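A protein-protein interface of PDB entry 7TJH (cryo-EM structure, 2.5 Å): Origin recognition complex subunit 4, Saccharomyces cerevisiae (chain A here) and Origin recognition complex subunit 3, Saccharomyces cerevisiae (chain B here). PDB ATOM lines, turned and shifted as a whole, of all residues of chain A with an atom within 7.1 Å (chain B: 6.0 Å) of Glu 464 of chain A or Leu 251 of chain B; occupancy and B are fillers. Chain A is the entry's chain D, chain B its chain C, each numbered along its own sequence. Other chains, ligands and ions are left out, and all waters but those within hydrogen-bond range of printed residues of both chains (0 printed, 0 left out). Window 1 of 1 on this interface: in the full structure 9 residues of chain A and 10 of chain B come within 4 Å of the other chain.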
ATOM      1  N   PHE A 411     -16.492  22.829  -1.220  1.00  0.00           N
ATOM      2  CA  PHE A 411     -17.107  24.129  -1.462  1.00  0.00           C
ATOM      3  C   PHE A 411     -18.632  24.056  -1.401  1.00  0.00           C
ATOM      4  O   PHE A 411     -19.282  24.989  -0.915  1.00  0.00           O
ATOM      5  CB  PHE A 411     -16.627  24.649  -2.817  1.00  0.00           C
ATOM      6  CG  PHE A 411     -17.190  25.976  -3.205  1.00  0.00           C
ATOM      7  CD1 PHE A 411     -16.703  27.140  -2.636  1.00  0.00           C
ATOM      8  CD2 PHE A 411     -18.188  26.066  -4.163  1.00  0.00           C
ATOM      9  CE1 PHE A 411     -17.211  28.366  -2.999  1.00  0.00           C
ATOM     10  CE2 PHE A 411     -18.705  27.291  -4.531  1.00  0.00           C
ATOM     11  CZ  PHE A 411     -18.214  28.444  -3.947  1.00  0.00           C
ATOM     12  N   VAL A 459     -18.651  33.443  -4.354  1.00  0.00           N
ATOM     13  CA  VAL A 459     -18.011  32.855  -3.185  1.00  0.00           C
ATOM     14  C   VAL A 459     -16.750  32.085  -3.585  1.00  0.00           C
ATOM     15  O   VAL A 459     -15.896  31.819  -2.732  1.00  0.00           O
ATOM     16  CB  VAL A 459     -19.107  32.051  -2.449  1.00  0.00           C
ATOM     17  CG1 VAL A 459     -18.603  31.239  -1.261  1.00  0.00           C
ATOM     18  CG2 VAL A 459     -20.158  33.005  -1.942  1.00  0.00           C
ATOM     19  N   LYS A 460     -16.584  31.794  -4.880  1.00  0.00           N
ATOM     20  CA  LYS A 460     -15.392  31.112  -5.384  1.00  0.00           C
ATOM     21  C   LYS A 460     -14.122  31.923  -5.132  1.00  0.00           C
ATOM     22  O   LYS A 460     -13.083  31.365  -4.754  1.00  0.00           O
ATOM     23  CB  LYS A 460     -15.578  30.831  -6.877  1.00  0.00           C
ATOM     24  CG  LYS A 460     -14.365  30.302  -7.624  1.00  0.00           C
ATOM     25  CD  LYS A 460     -14.757  29.934  -9.048  1.00  0.00           C
ATOM     26  CE  LYS A 460     -13.606  29.325  -9.834  1.00  0.00           C
ATOM     27  NZ  LYS A 460     -12.725  30.367 -10.424  1.00  0.00           N
ATOM     28  N   ASN A 461     -14.202  33.244  -5.310  1.00  0.00           N
ATOM     29  CA  ASN A 461     -13.075  34.130  -5.025  1.00  0.00           C
ATOM     30  C   ASN A 461     -12.724  34.130  -3.540  1.00  0.00           C
ATOM     31  O   ASN A 461     -11.541  34.093  -3.172  1.00  0.00           O
ATOM     32  CB  ASN A 461     -13.416  35.538  -5.510  1.00  0.00           C
ATOM     33  CG  ASN A 461     -12.225  36.464  -5.526  1.00  0.00           C
ATOM     34  OD1 ASN A 461     -11.308  36.300  -6.325  1.00  0.00           O
ATOM     35  ND2 ASN A 461     -12.241  37.457  -4.650  1.00  0.00           N
ATOM     36  N   VAL A 462     -13.746  34.145  -2.677  1.00  0.00           N
ATOM     37  CA  VAL A 462     -13.559  34.067  -1.228  1.00  0.00           C
ATOM     38  C   VAL A 462     -12.921  32.738  -0.840  1.00  0.00           C
ATOM     39  O   VAL A 462     -12.028  32.683   0.016  1.00  0.00           O
ATOM     40  CB  VAL A 462     -14.916  34.284  -0.525  1.00  0.00           C
ATOM     41  CG1 VAL A 462     -14.847  33.968   0.963  1.00  0.00           C
ATOM     42  CG2 VAL A 462     -15.406  35.699  -0.747  1.00  0.00           C
ATOM     43  N   TRP A 463     -13.362  31.653  -1.478  1.00  0.00           N
ATOM     44  CA  TRP A 463     -12.837  30.320  -1.210  1.00  0.00           C
ATOM     45  C   TRP A 463     -11.369  30.210  -1.602  1.00  0.00           C
ATOM     46  O   TRP A 463     -10.561  29.640  -0.858  1.00  0.00           O
ATOM     47  CB  TRP A 463     -13.672  29.289  -1.966  1.00  0.00           C
ATOM     48  CG  TRP A 463     -13.383  27.876  -1.622  1.00  0.00           C
ATOM     49  CD1 TRP A 463     -12.541  27.025  -2.277  1.00  0.00           C
ATOM     50  CD2 TRP A 463     -13.947  27.133  -0.544  1.00  0.00           C
ATOM     51  NE1 TRP A 463     -12.544  25.797  -1.666  1.00  0.00           N
ATOM     52  CE2 TRP A 463     -13.401  25.837  -0.600  1.00  0.00           C
ATOM     53  CE3 TRP A 463     -14.863  27.437   0.465  1.00  0.00           C
ATOM     54  CZ2 TRP A 463     -13.742  24.848   0.314  1.00  0.00           C
ATOM     55  CZ3 TRP A 463     -15.194  26.459   1.370  1.00  0.00           C
ATOM     56  CH2 TRP A 463     -14.640  25.179   1.287  1.00  0.00           C
ATOM     57  N   GLU A 464     -11.010  30.765  -2.763  1.00  0.00           N
ATOM     58  CA  GLU A 464      -9.615  30.771  -3.194  1.00  0.00           C
ATOM     59  C   GLU A 464      -8.752  31.629  -2.276  1.00  0.00           C
ATOM     60  O   GLU A 464      -7.597  31.279  -2.002  1.00  0.00           O
ATOM     61  CB  GLU A 464      -9.513  31.252  -4.640  1.00  0.00           C
ATOM     62  CG  GLU A 464      -9.891  30.202  -5.672  1.00  0.00           C
ATOM     63  CD  GLU A 464     -10.461  30.803  -6.946  1.00  0.00           C
ATOM     64  OE1 GLU A 464     -10.615  32.039  -7.006  1.00  0.00           O
ATOM     65  OE2 GLU A 464     -10.756  30.037  -7.887  1.00  0.00           O
ATOM     66  N   ASN A 465      -9.294  32.753  -1.791  1.00  0.00           N
ATOM     67  CA  ASN A 465      -8.564  33.579  -0.831  1.00  0.00           C
ATOM     68  C   ASN A 465      -8.352  32.848   0.491  1.00  0.00           C
ATOM     69  O   ASN A 465      -7.290  32.972   1.112  1.00  0.00           O
ATOM     70  CB  ASN A 465      -9.302  34.895  -0.598  1.00  0.00           C
ATOM     71  CG  ASN A 465      -9.265  35.805  -1.806  1.00  0.00           C
ATOM     72  OD1 ASN A 465      -8.439  35.637  -2.701  1.00  0.00           O
ATOM     73  ND2 ASN A 465     -10.165  36.778  -1.841  1.00  0.00           N
ATOM     74  N   LEU A 466      -9.355  32.088   0.935  1.00  0.00           N
ATOM     75  CA  LEU A 466      -9.225  31.323   2.172  1.00  0.00           C
ATOM     76  C   LEU A 466      -8.218  30.188   2.027  1.00  0.00           C
ATOM     77  O   LEU A 466      -7.502  29.865   2.980  1.00  0.00           O
ATOM     78  CB  LEU A 466     -10.588  30.782   2.597  1.00  0.00           C
ATOM     79  CG  LEU A 466     -11.530  31.776   3.273  1.00  0.00           C
ATOM     80  CD1 LEU A 466     -12.922  31.185   3.407  1.00  0.00           C
ATOM     81  CD2 LEU A 466     -10.989  32.192   4.627  1.00  0.00           C
ATOM     82  N   VAL A 467      -8.164  29.562   0.848  1.00  0.00           N
ATOM     83  CA  VAL A 467      -7.162  28.529   0.589  1.00  0.00           C
ATOM     84  C   VAL A 467      -5.760  29.135   0.552  1.00  0.00           C
ATOM     85  O   VAL A 467      -4.815  28.580   1.128  1.00  0.00           O
ATOM     86  CB  VAL A 467      -7.505  27.776  -0.714  1.00  0.00           C
ATOM     87  CG1 VAL A 467      -6.339  26.912  -1.187  1.00  0.00           C
ATOM     88  CG2 VAL A 467      -8.739  26.915  -0.515  1.00  0.00           C
ATOM     89  N   GLN A 468      -5.610  30.293  -0.097  1.00  0.00           N
ATOM     90  CA  GLN A 468      -4.309  30.945  -0.214  1.00  0.00           C
ATOM     91  C   GLN A 468      -3.799  31.450   1.135  1.00  0.00           C
ATOM     92  O   GLN A 468      -2.588  31.439   1.383  1.00  0.00           O
ATOM     93  CB  GLN A 468      -4.404  32.089  -1.231  1.00  0.00           C
ATOM     94  CG  GLN A 468      -3.174  32.984  -1.396  1.00  0.00           C
ATOM     95  CD  GLN A 468      -2.072  32.359  -2.242  1.00  0.00           C
ATOM     96  OE1 GLN A 468      -1.529  31.301  -1.915  1.00  0.00           O
ATOM     97  NE2 GLN A 468      -1.735  33.021  -3.341  1.00  0.00           N
ATOM     98  N   LEU A 469      -4.698  31.848   2.033  1.00  0.00           N
ATOM     99  CA  LEU A 469      -4.320  32.351   3.348  1.00  0.00           C
ATOM    100  C   LEU A 469      -4.095  31.247   4.379  1.00  0.00           C
ATOM    101  O   LEU A 469      -4.055  31.564   5.573  1.00  0.00           O
ATOM    102  CB  LEU A 469      -5.385  33.318   3.866  1.00  0.00           C
ATOM    103  CG  LEU A 469      -5.342  34.774   3.401  1.00  0.00           C
ATOM    104  CD1 LEU A 469      -6.270  35.607   4.259  1.00  0.00           C
ATOM    105  CD2 LEU A 469      -3.931  35.327   3.447  1.00  0.00           C
ATOM    106  N   ASP A 470      -3.972  29.989   3.934  1.00  0.00           N
ATOM    107  CA  ASP A 470      -3.632  28.824   4.764  1.00  0.00           C
ATOM    108  C   ASP A 470      -4.678  28.613   5.868  1.00  0.00           C
ATOM    109  O   ASP A 470      -4.365  28.381   7.037  1.00  0.00           O
ATOM    110  CB  ASP A 470      -2.200  28.947   5.318  1.00  0.00           C
ATOM    111  CG  ASP A 470      -1.681  27.657   5.947  1.00  0.00           C
ATOM    112  OD1 ASP A 470      -2.198  26.574   5.598  1.00  0.00           O
ATOM    113  OD2 ASP A 470      -0.759  27.731   6.789  1.00  0.00           O
ATOM    114  N   PHE A 472      -7.554  26.568   4.824  1.00  0.00           N
ATOM    115  CA  PHE A 472      -7.884  25.214   4.415  1.00  0.00           C
ATOM    116  C   PHE A 472      -6.658  24.579   3.777  1.00  0.00           C
ATOM    117  O   PHE A 472      -5.878  25.252   3.098  1.00  0.00           O
ATOM    118  CB  PHE A 472      -9.053  25.152   3.404  1.00  0.00           C
ATOM    119  CG  PHE A 472     -10.245  26.010   3.751  1.00  0.00           C
ATOM    120  CD1 PHE A 472     -10.699  26.127   5.058  1.00  0.00           C
ATOM    121  CD2 PHE A 472     -10.941  26.667   2.746  1.00  0.00           C
ATOM    122  CE1 PHE A 472     -11.796  26.905   5.356  1.00  0.00           C
ATOM    123  CE2 PHE A 472     -12.046  27.443   3.039  1.00  0.00           C
ATOM    124  CZ  PHE A 472     -12.473  27.564   4.347  1.00  0.00           C
ATOM    125  N   PHE A 502     -13.389  22.269  -8.917  1.00  0.00           N
ATOM    126  CA  PHE A 502     -12.954  22.872  -7.657  1.00  0.00           C
ATOM    127  C   PHE A 502     -13.985  22.744  -6.541  1.00  0.00           C
ATOM    128  O   PHE A 502     -13.616  22.830  -5.366  1.00  0.00           O
ATOM    129  CB  PHE A 502     -12.606  24.352  -7.878  1.00  0.00           C
ATOM    130  CG  PHE A 502     -13.774  25.291  -7.697  1.00  0.00           C
ATOM    131  CD1 PHE A 502     -14.742  25.403  -8.683  1.00  0.00           C
ATOM    132  CD2 PHE A 502     -13.901  26.064  -6.544  1.00  0.00           C
ATOM    133  CE1 PHE A 502     -15.819  26.260  -8.523  1.00  0.00           C
ATOM    134  CE2 PHE A 502     -14.984  26.910  -6.372  1.00  0.00           C
ATOM    135  CZ  PHE A 502     -15.940  27.010  -7.362  1.00  0.00           C
ATOM    136  N   ARG A 505     -13.352  19.345  -4.414  1.00  0.00           N
ATOM    137  CA  ARG A 505     -12.068  19.084  -3.775  1.00  0.00           C
ATOM    138  C   ARG A 505     -12.231  19.009  -2.263  1.00  0.00           C
ATOM    139  O   ARG A 505     -12.876  19.867  -1.654  1.00  0.00           O
ATOM    140  CB  ARG A 505     -11.063  20.173  -4.140  1.00  0.00           C
ATOM    141  CG  ARG A 505     -10.536  20.091  -5.554  1.00  0.00           C
ATOM    142  CD  ARG A 505      -9.421  21.096  -5.782  1.00  0.00           C
ATOM    143  NE  ARG A 505      -9.433  21.615  -7.145  1.00  0.00           N
ATOM    144  CZ  ARG A 505      -9.193  22.878  -7.468  1.00  0.00           C
ATOM    145  NH1 ARG A 505      -8.884  23.780  -6.551  1.00  0.00           N
ATOM    146  NH2 ARG A 505      -9.258  23.246  -8.744  1.00  0.00           N
ATOM    147  N   PHE B 213      -5.090  22.246 -15.653  1.00  0.00           N
ATOM    148  CA  PHE B 213      -5.389  23.666 -15.519  1.00  0.00           C
ATOM    149  C   PHE B 213      -4.640  24.324 -14.371  1.00  0.00           C
ATOM    150  O   PHE B 213      -4.436  25.540 -14.406  1.00  0.00           O
ATOM    151  CB  PHE B 213      -6.894  23.869 -15.365  1.00  0.00           C
ATOM    152  CG  PHE B 213      -7.634  23.841 -16.667  1.00  0.00           C
ATOM    153  CD1 PHE B 213      -7.648  24.955 -17.489  1.00  0.00           C
ATOM    154  CD2 PHE B 213      -8.305  22.700 -17.074  1.00  0.00           C
ATOM    155  CE1 PHE B 213      -8.326  24.936 -18.697  1.00  0.00           C
ATOM    156  CE2 PHE B 213      -8.983  22.672 -18.278  1.00  0.00           C
ATOM    157  CZ  PHE B 213      -8.993  23.792 -19.091  1.00  0.00           C
ATOM    158  N   ASN B 214      -4.219  23.553 -13.366  1.00  0.00           N
ATOM    159  CA  ASN B 214      -3.362  24.094 -12.315  1.00  0.00           C
ATOM    160  C   ASN B 214      -2.001  24.500 -12.869  1.00  0.00           C
ATOM    161  O   ASN B 214      -1.496  25.592 -12.567  1.00  0.00           O
ATOM    162  CB  ASN B 214      -3.214  23.057 -11.201  1.00  0.00           C
ATOM    163  CG  ASN B 214      -2.557  23.619  -9.965  1.00  0.00           C
ATOM    164  OD1 ASN B 214      -2.947  24.673  -9.462  1.00  0.00           O
ATOM    165  ND2 ASN B 214      -1.551  22.918  -9.465  1.00  0.00           N
ATOM    166  N   LEU B 216      -1.370  25.204 -16.072  1.00  0.00           N
ATOM    167  CA  LEU B 216      -1.579  26.312 -17.000  1.00  0.00           C
ATOM    168  C   LEU B 216      -1.795  27.629 -16.259  1.00  0.00           C
ATOM    169  O   LEU B 216      -1.274  28.671 -16.675  1.00  0.00           O
ATOM    170  CB  LEU B 216      -2.761  26.000 -17.915  1.00  0.00           C
ATOM    171  CG  LEU B 216      -3.217  27.079 -18.895  1.00  0.00           C
ATOM    172  CD1 LEU B 216      -2.207  27.246 -20.015  1.00  0.00           C
ATOM    173  CD2 LEU B 216      -4.591  26.737 -19.442  1.00  0.00           C
ATOM    174  N   ASP B 217      -2.537  27.584 -15.147  1.00  0.00           N
ATOM    175  CA  ASP B 217      -2.750  28.761 -14.311  1.00  0.00           C
ATOM    176  C   ASP B 217      -1.437  29.277 -13.731  1.00  0.00           C
ATOM    177  O   ASP B 217      -1.159  30.484 -13.767  1.00  0.00           O
ATOM    178  CB  ASP B 217      -3.732  28.414 -13.190  1.00  0.00           C
ATOM    179  CG  ASP B 217      -4.533  29.609 -12.716  1.00  0.00           C
ATOM    180  OD1 ASP B 217      -3.931  30.654 -12.408  1.00  0.00           O
ATOM    181  OD2 ASP B 217      -5.771  29.497 -12.624  1.00  0.00           O
ATOM    182  N   ILE B 220       0.645  30.895 -16.518  1.00  0.00           N
ATOM    183  CA  ILE B 220       0.165  32.229 -16.880  1.00  0.00           C
ATOM    184  C   ILE B 220       0.560  33.250 -15.814  1.00  0.00           C
ATOM    185  O   ILE B 220       0.994  34.368 -16.133  1.00  0.00           O
ATOM    186  CB  ILE B 220      -1.359  32.193 -17.123  1.00  0.00           C
ATOM    187  CG1 ILE B 220      -1.673  31.415 -18.402  1.00  0.00           C
ATOM    188  CG2 ILE B 220      -1.951  33.590 -17.233  1.00  0.00           C
ATOM    189  CD1 ILE B 220      -3.088  30.891 -18.458  1.00  0.00           C
ATOM    190  N   ASN B 246     -16.464  26.270 -19.168  1.00  0.00           N
ATOM    191  CA  ASN B 246     -15.737  25.151 -18.573  1.00  0.00           C
ATOM    192  C   ASN B 246     -14.332  25.561 -18.146  1.00  0.00           C
ATOM    193  O   ASN B 246     -13.890  25.236 -17.038  1.00  0.00           O
ATOM    194  CB  ASN B 246     -15.678  23.979 -19.553  1.00  0.00           C
ATOM    195  CG  ASN B 246     -16.981  23.210 -19.618  1.00  0.00           C
ATOM    196  OD1 ASN B 246     -17.908  23.602 -20.324  1.00  0.00           O
ATOM    197  ND2 ASN B 246     -17.053  22.102 -18.890  1.00  0.00           N
ATOM    198  N   ILE B 247     -13.620  26.295 -19.004  1.00  0.00           N
ATOM    199  CA  ILE B 247     -12.278  26.733 -18.638  1.00  0.00           C
ATOM    200  C   ILE B 247     -12.321  27.915 -17.676  1.00  0.00           C
ATOM    201  O   ILE B 247     -11.295  28.239 -17.065  1.00  0.00           O
ATOM    202  CB  ILE B 247     -11.443  27.037 -19.898  1.00  0.00           C
ATOM    203  CG1 ILE B 247     -11.737  28.424 -20.485  1.00  0.00           C
ATOM    204  CG2 ILE B 247     -11.669  25.956 -20.950  1.00  0.00           C
ATOM    205  CD1 ILE B 247     -10.638  29.471 -20.261  1.00  0.00           C
ATOM    206  N   GLU B 248     -13.475  28.572 -17.529  1.00  0.00           N
ATOM    207  CA  GLU B 248     -13.595  29.611 -16.512  1.00  0.00           C
ATOM    208  C   GLU B 248     -13.569  29.030 -15.100  1.00  0.00           C
ATOM    209  O   GLU B 248     -12.880  29.559 -14.223  1.00  0.00           O
ATOM    210  CB  GLU B 248     -14.872  30.417 -16.735  1.00  0.00           C
ATOM    211  CG  GLU B 248     -14.850  31.786 -16.086  1.00  0.00           C
ATOM    212  CD  GLU B 248     -15.644  32.812 -16.873  1.00  0.00           C
ATOM    213  OE1 GLU B 248     -16.823  32.547 -17.187  1.00  0.00           O
ATOM    214  OE2 GLU B 248     -15.084  33.882 -17.177  1.00  0.00           O
ATOM    215  N   LYS B 249     -14.296  27.941 -14.859  1.00  0.00           N
ATOM    216  CA  LYS B 249     -14.349  27.391 -13.508  1.00  0.00           C
ATOM    217  C   LYS B 249     -13.137  26.543 -13.149  1.00  0.00           C
ATOM    218  O   LYS B 249     -12.998  26.164 -11.982  1.00  0.00           O
ATOM    219  CB  LYS B 249     -15.626  26.573 -13.310  1.00  0.00           C
ATOM    220  CG  LYS B 249     -16.849  27.149 -14.010  1.00  0.00           C
ATOM    221  CD  LYS B 249     -17.958  26.121 -14.259  1.00  0.00           C
ATOM    222  CE  LYS B 249     -18.327  25.246 -13.050  1.00  0.00           C
ATOM    223  NZ  LYS B 249     -18.423  25.949 -11.731  1.00  0.00           N
ATOM    224  N   ASN B 250     -12.264  26.238 -14.104  1.00  0.00           N
ATOM    225  CA  ASN B 250     -11.047  25.485 -13.834  1.00  0.00           C
ATOM    226  C   ASN B 250      -9.847  26.381 -13.565  1.00  0.00           C
ATOM    227  O   ASN B 250      -8.747  25.868 -13.343  1.00  0.00           O
ATOM    228  CB  ASN B 250     -10.738  24.543 -15.002  1.00  0.00           C
ATOM    229  CG  ASN B 250     -11.854  23.552 -15.265  1.00  0.00           C
ATOM    230  OD1 ASN B 250     -12.746  23.372 -14.439  1.00  0.00           O
ATOM    231  ND2 ASN B 250     -11.809  22.903 -16.424  1.00  0.00           N
ATOM    232  N   LEU B 251     -10.028  27.698 -13.579  1.00  0.00           N
ATOM    233  CA  LEU B 251      -8.957  28.643 -13.317  1.00  0.00           C
ATOM    234  C   LEU B 251      -9.311  29.513 -12.119  1.00  0.00           C
ATOM    235  O   LEU B 251     -10.481  29.667 -11.757  1.00  0.00           O
ATOM    236  CB  LEU B 251      -8.676  29.533 -14.535  1.00  0.00           C
ATOM    237  CG  LEU B 251      -8.103  28.879 -15.793  1.00  0.00           C
ATOM    238  CD1 LEU B 251      -7.969  29.902 -16.906  1.00  0.00           C
ATOM    239  CD2 LEU B 251      -6.767  28.212 -15.514  1.00  0.00           C
ATOM    240  N   ARG B 252      -8.277  30.078 -11.502  1.00  0.00           N
ATOM    241  CA  ARG B 252      -8.468  30.974 -10.370  1.00  0.00           C
ATOM    242  C   ARG B 252      -9.094  32.287 -10.829  1.00  0.00           C
ATOM    243  O   ARG B 252      -8.936  32.708 -11.975  1.00  0.00           O
ATOM    244  CB  ARG B 252      -7.136  31.240  -9.668  1.00  0.00           C
ATOM    245  CG  ARG B 252      -6.899  30.361  -8.457  1.00  0.00           C
ATOM    246  CD  ARG B 252      -5.631  29.531  -8.606  1.00  0.00           C
ATOM    247  NE  ARG B 252      -4.429  30.271  -8.243  1.00  0.00           N
ATOM    248  CZ  ARG B 252      -3.192  29.849  -8.474  1.00  0.00           C
ATOM    249  NH1 ARG B 252      -2.957  28.715  -9.117  1.00  0.00           N
ATOM    250  NH2 ARG B 252      -2.166  30.579  -8.047  1.00  0.00           N
ATOM    251  N   GLN B 253      -9.818  32.928  -9.907  1.00  0.00           N
ATOM    252  CA  GLN B 253     -10.570  34.134 -10.237  1.00  0.00           C
ATOM    253  C   GLN B 253      -9.656  35.317 -10.532  1.00  0.00           C
ATOM    254  O   GLN B 253     -10.001  36.174 -11.353  1.00  0.00           O
ATOM    255  CB  GLN B 253     -11.533  34.469  -9.099  1.00  0.00           C
ATOM    256  CG  GLN B 253     -12.642  35.423  -9.483  1.00  0.00           C
ATOM    257  CD  GLN B 253     -13.429  34.944 -10.680  1.00  0.00           C
ATOM    258  OE1 GLN B 253     -13.597  35.674 -11.650  1.00  0.00           O
ATOM    259  NE2 GLN B 253     -13.932  33.718 -10.609  1.00  0.00           N
ATOM    260  N   SER B 254      -8.495  35.383  -9.878  1.00  0.00           N
ATOM    261  CA  SER B 254      -7.512  36.409 -10.210  1.00  0.00           C
ATOM    262  C   SER B 254      -6.925  36.195 -11.602  1.00  0.00           C
ATOM    263  O   SER B 254      -6.639  37.169 -12.306  1.00  0.00           O
ATOM    264  CB  SER B 254      -6.409  36.433  -9.154  1.00  0.00           C
ATOM    265  OG  SER B 254      -5.791  35.167  -9.038  1.00  0.00           O
ATOM    266  N   THR B 255      -6.758  34.938 -12.018  1.00  0.00           N
ATOM    267  CA  THR B 255      -6.301  34.643 -13.373  1.00  0.00           C
ATOM    268  C   THR B 255      -7.350  35.047 -14.406  1.00  0.00           C
ATOM    269  O   THR B 255      -7.009  35.577 -15.472  1.00  0.00           O
ATOM    270  CB  THR B 255      -5.946  33.155 -13.478  1.00  0.00           C
ATOM    271  OG1 THR B 255      -4.882  32.859 -12.567  1.00  0.00           O
ATOM    272  CG2 THR B 255      -5.499  32.768 -14.887  1.00  0.00           C
ATOM    273  N   ILE B 256      -8.632  34.825 -14.090  1.00  0.00           N
ATOM    274  CA  ILE B 256      -9.729  35.282 -14.944  1.00  0.00           C
ATOM    275  C   ILE B 256      -9.738  36.803 -15.042  1.00  0.00           C
ATOM    276  O   ILE B 256      -9.888  37.366 -16.133  1.00  0.00           O
ATOM    277  CB  ILE B 256     -11.071  34.744 -14.413  1.00  0.00           C
ATOM    278  CG1 ILE B 256     -11.097  33.219 -14.448  1.00  0.00           C
ATOM    279  CG2 ILE B 256     -12.250  35.305 -15.205  1.00  0.00           C
ATOM    280  CD1 ILE B 256     -12.041  32.625 -13.436  1.00  0.00           C
ATOM    281  N   LEU B 259      -6.952  37.808 -17.336  1.00  0.00           N
ATOM    282  CA  LEU B 259      -7.266  37.532 -18.735  1.00  0.00           C
ATOM    283  C   LEU B 259      -8.365  38.432 -19.286  1.00  0.00           C
ATOM    284  O   LEU B 259      -8.433  38.630 -20.502  1.00  0.00           O
ATOM    285  CB  LEU B 259      -7.681  36.070 -18.907  1.00  0.00           C
ATOM    286  CG  LEU B 259      -6.605  34.991 -18.779  1.00  0.00           C
ATOM    287  CD1 LEU B 259      -7.194  33.629 -19.088  1.00  0.00           C
ATOM    288  CD2 LEU B 259      -5.418  35.288 -19.677  1.00  0.00           C
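The side-chain carboxylate (OE1) of Glu 464 of chain A lies within hydrogen-bond range of the backbone NH (N) of Gln 253 of chain B, 3.1 Å away. The side-chain amino group (NZ) of Lys 460 of chain A is in hydrogen-bond range of the backbone carbonyl oxygen (O) of Leu 251 of chain B.
The side-chain carboxylate (OE2) of Glu 464 of chain A lies within salt-bridge range of the side-chain amino group (NZ) of Lys 460 of chain A. OD1 of Asp 217 of chain B is in salt-bridge range of NH1 of Arg 252 of chain B, 3.9 Å away. O of Asn 461 of chain A lies close to ND2 of Asn 465 of chain A (3.3 Å).
Glu 248 of chain B touches Lys 460 of chain A (O to NZ, 3.9 Å). Lys 460 of chain A touches Lys 249 of chain B (CE to O, 3.9 Å). Gln 253 of chain B touches Lys 460 of chain A. Ile 256 of chain B touches Lys 460 of chain A. CB of Gln 253 of chain B touches OD1 of Asn 461 of chain A, at 3.3 Å. OE2 of Glu 464 of chain A touches O of Leu 251 of chain B, at 3.9 Å. Arg 252 of chain B touches Glu 464 of chain A (CA to OE2, 3.5 Å). CD1 of Phe 502 of chain A touches O of Lys 249 of chain B (3.8 Å).
Glu 464 of chain A touches three residues of chain B. Of the printed residues of chain A, Leu 251 of chain B touches Lys 460 (2.7 Å) and Glu 464 (3.9 Å). Printed residues of chain B within 4 Å of Asn 461 of chain A: Gln 253 (3.3 Å). Of the printed residues of chain A, Lys 249 of chain B touches Lys 460 (3.9 Å) and Phe 502 (3.8 Å). Printed residues of chain A within 4 Å of Ile 256 of chain B: Lys 460 (3.8 Å). Ser 254 of chain B touches none of the printed residues of chain A. Thr 255 of chain B touches none of the printed residues of chain A. The nearest residue of chain B that does not touch Glu 464 of chain A is Ser 254 of chain B (4.9 Å). The nearest residue of chain A that does not touch Leu 251 of chain B is Arg 505 of chain A (6.6 Å).
Printed residues of chain A that touch a printed residue of chain B: Lys 460, Asn 461, Glu 464 and Phe 502. Of the 17 printed residues of chain B, 6 touch a printed residue of chain A. Printed residues of chain B that touch a printed residue of chain A: Glu 248, Lys 249, Leu 251, Arg 252, Gln 253 and Ile 256. Hydrophobic or aromatic side chains of chain B within 4 Å of the printed part of chain A: Ile 256. Among the printed residues, 10 pairs touch across the chains. Among the printed residues, no Asp or Glu carboxylate lies within 4 Å of a Lys or Arg side-chain nitrogen of the other chain.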
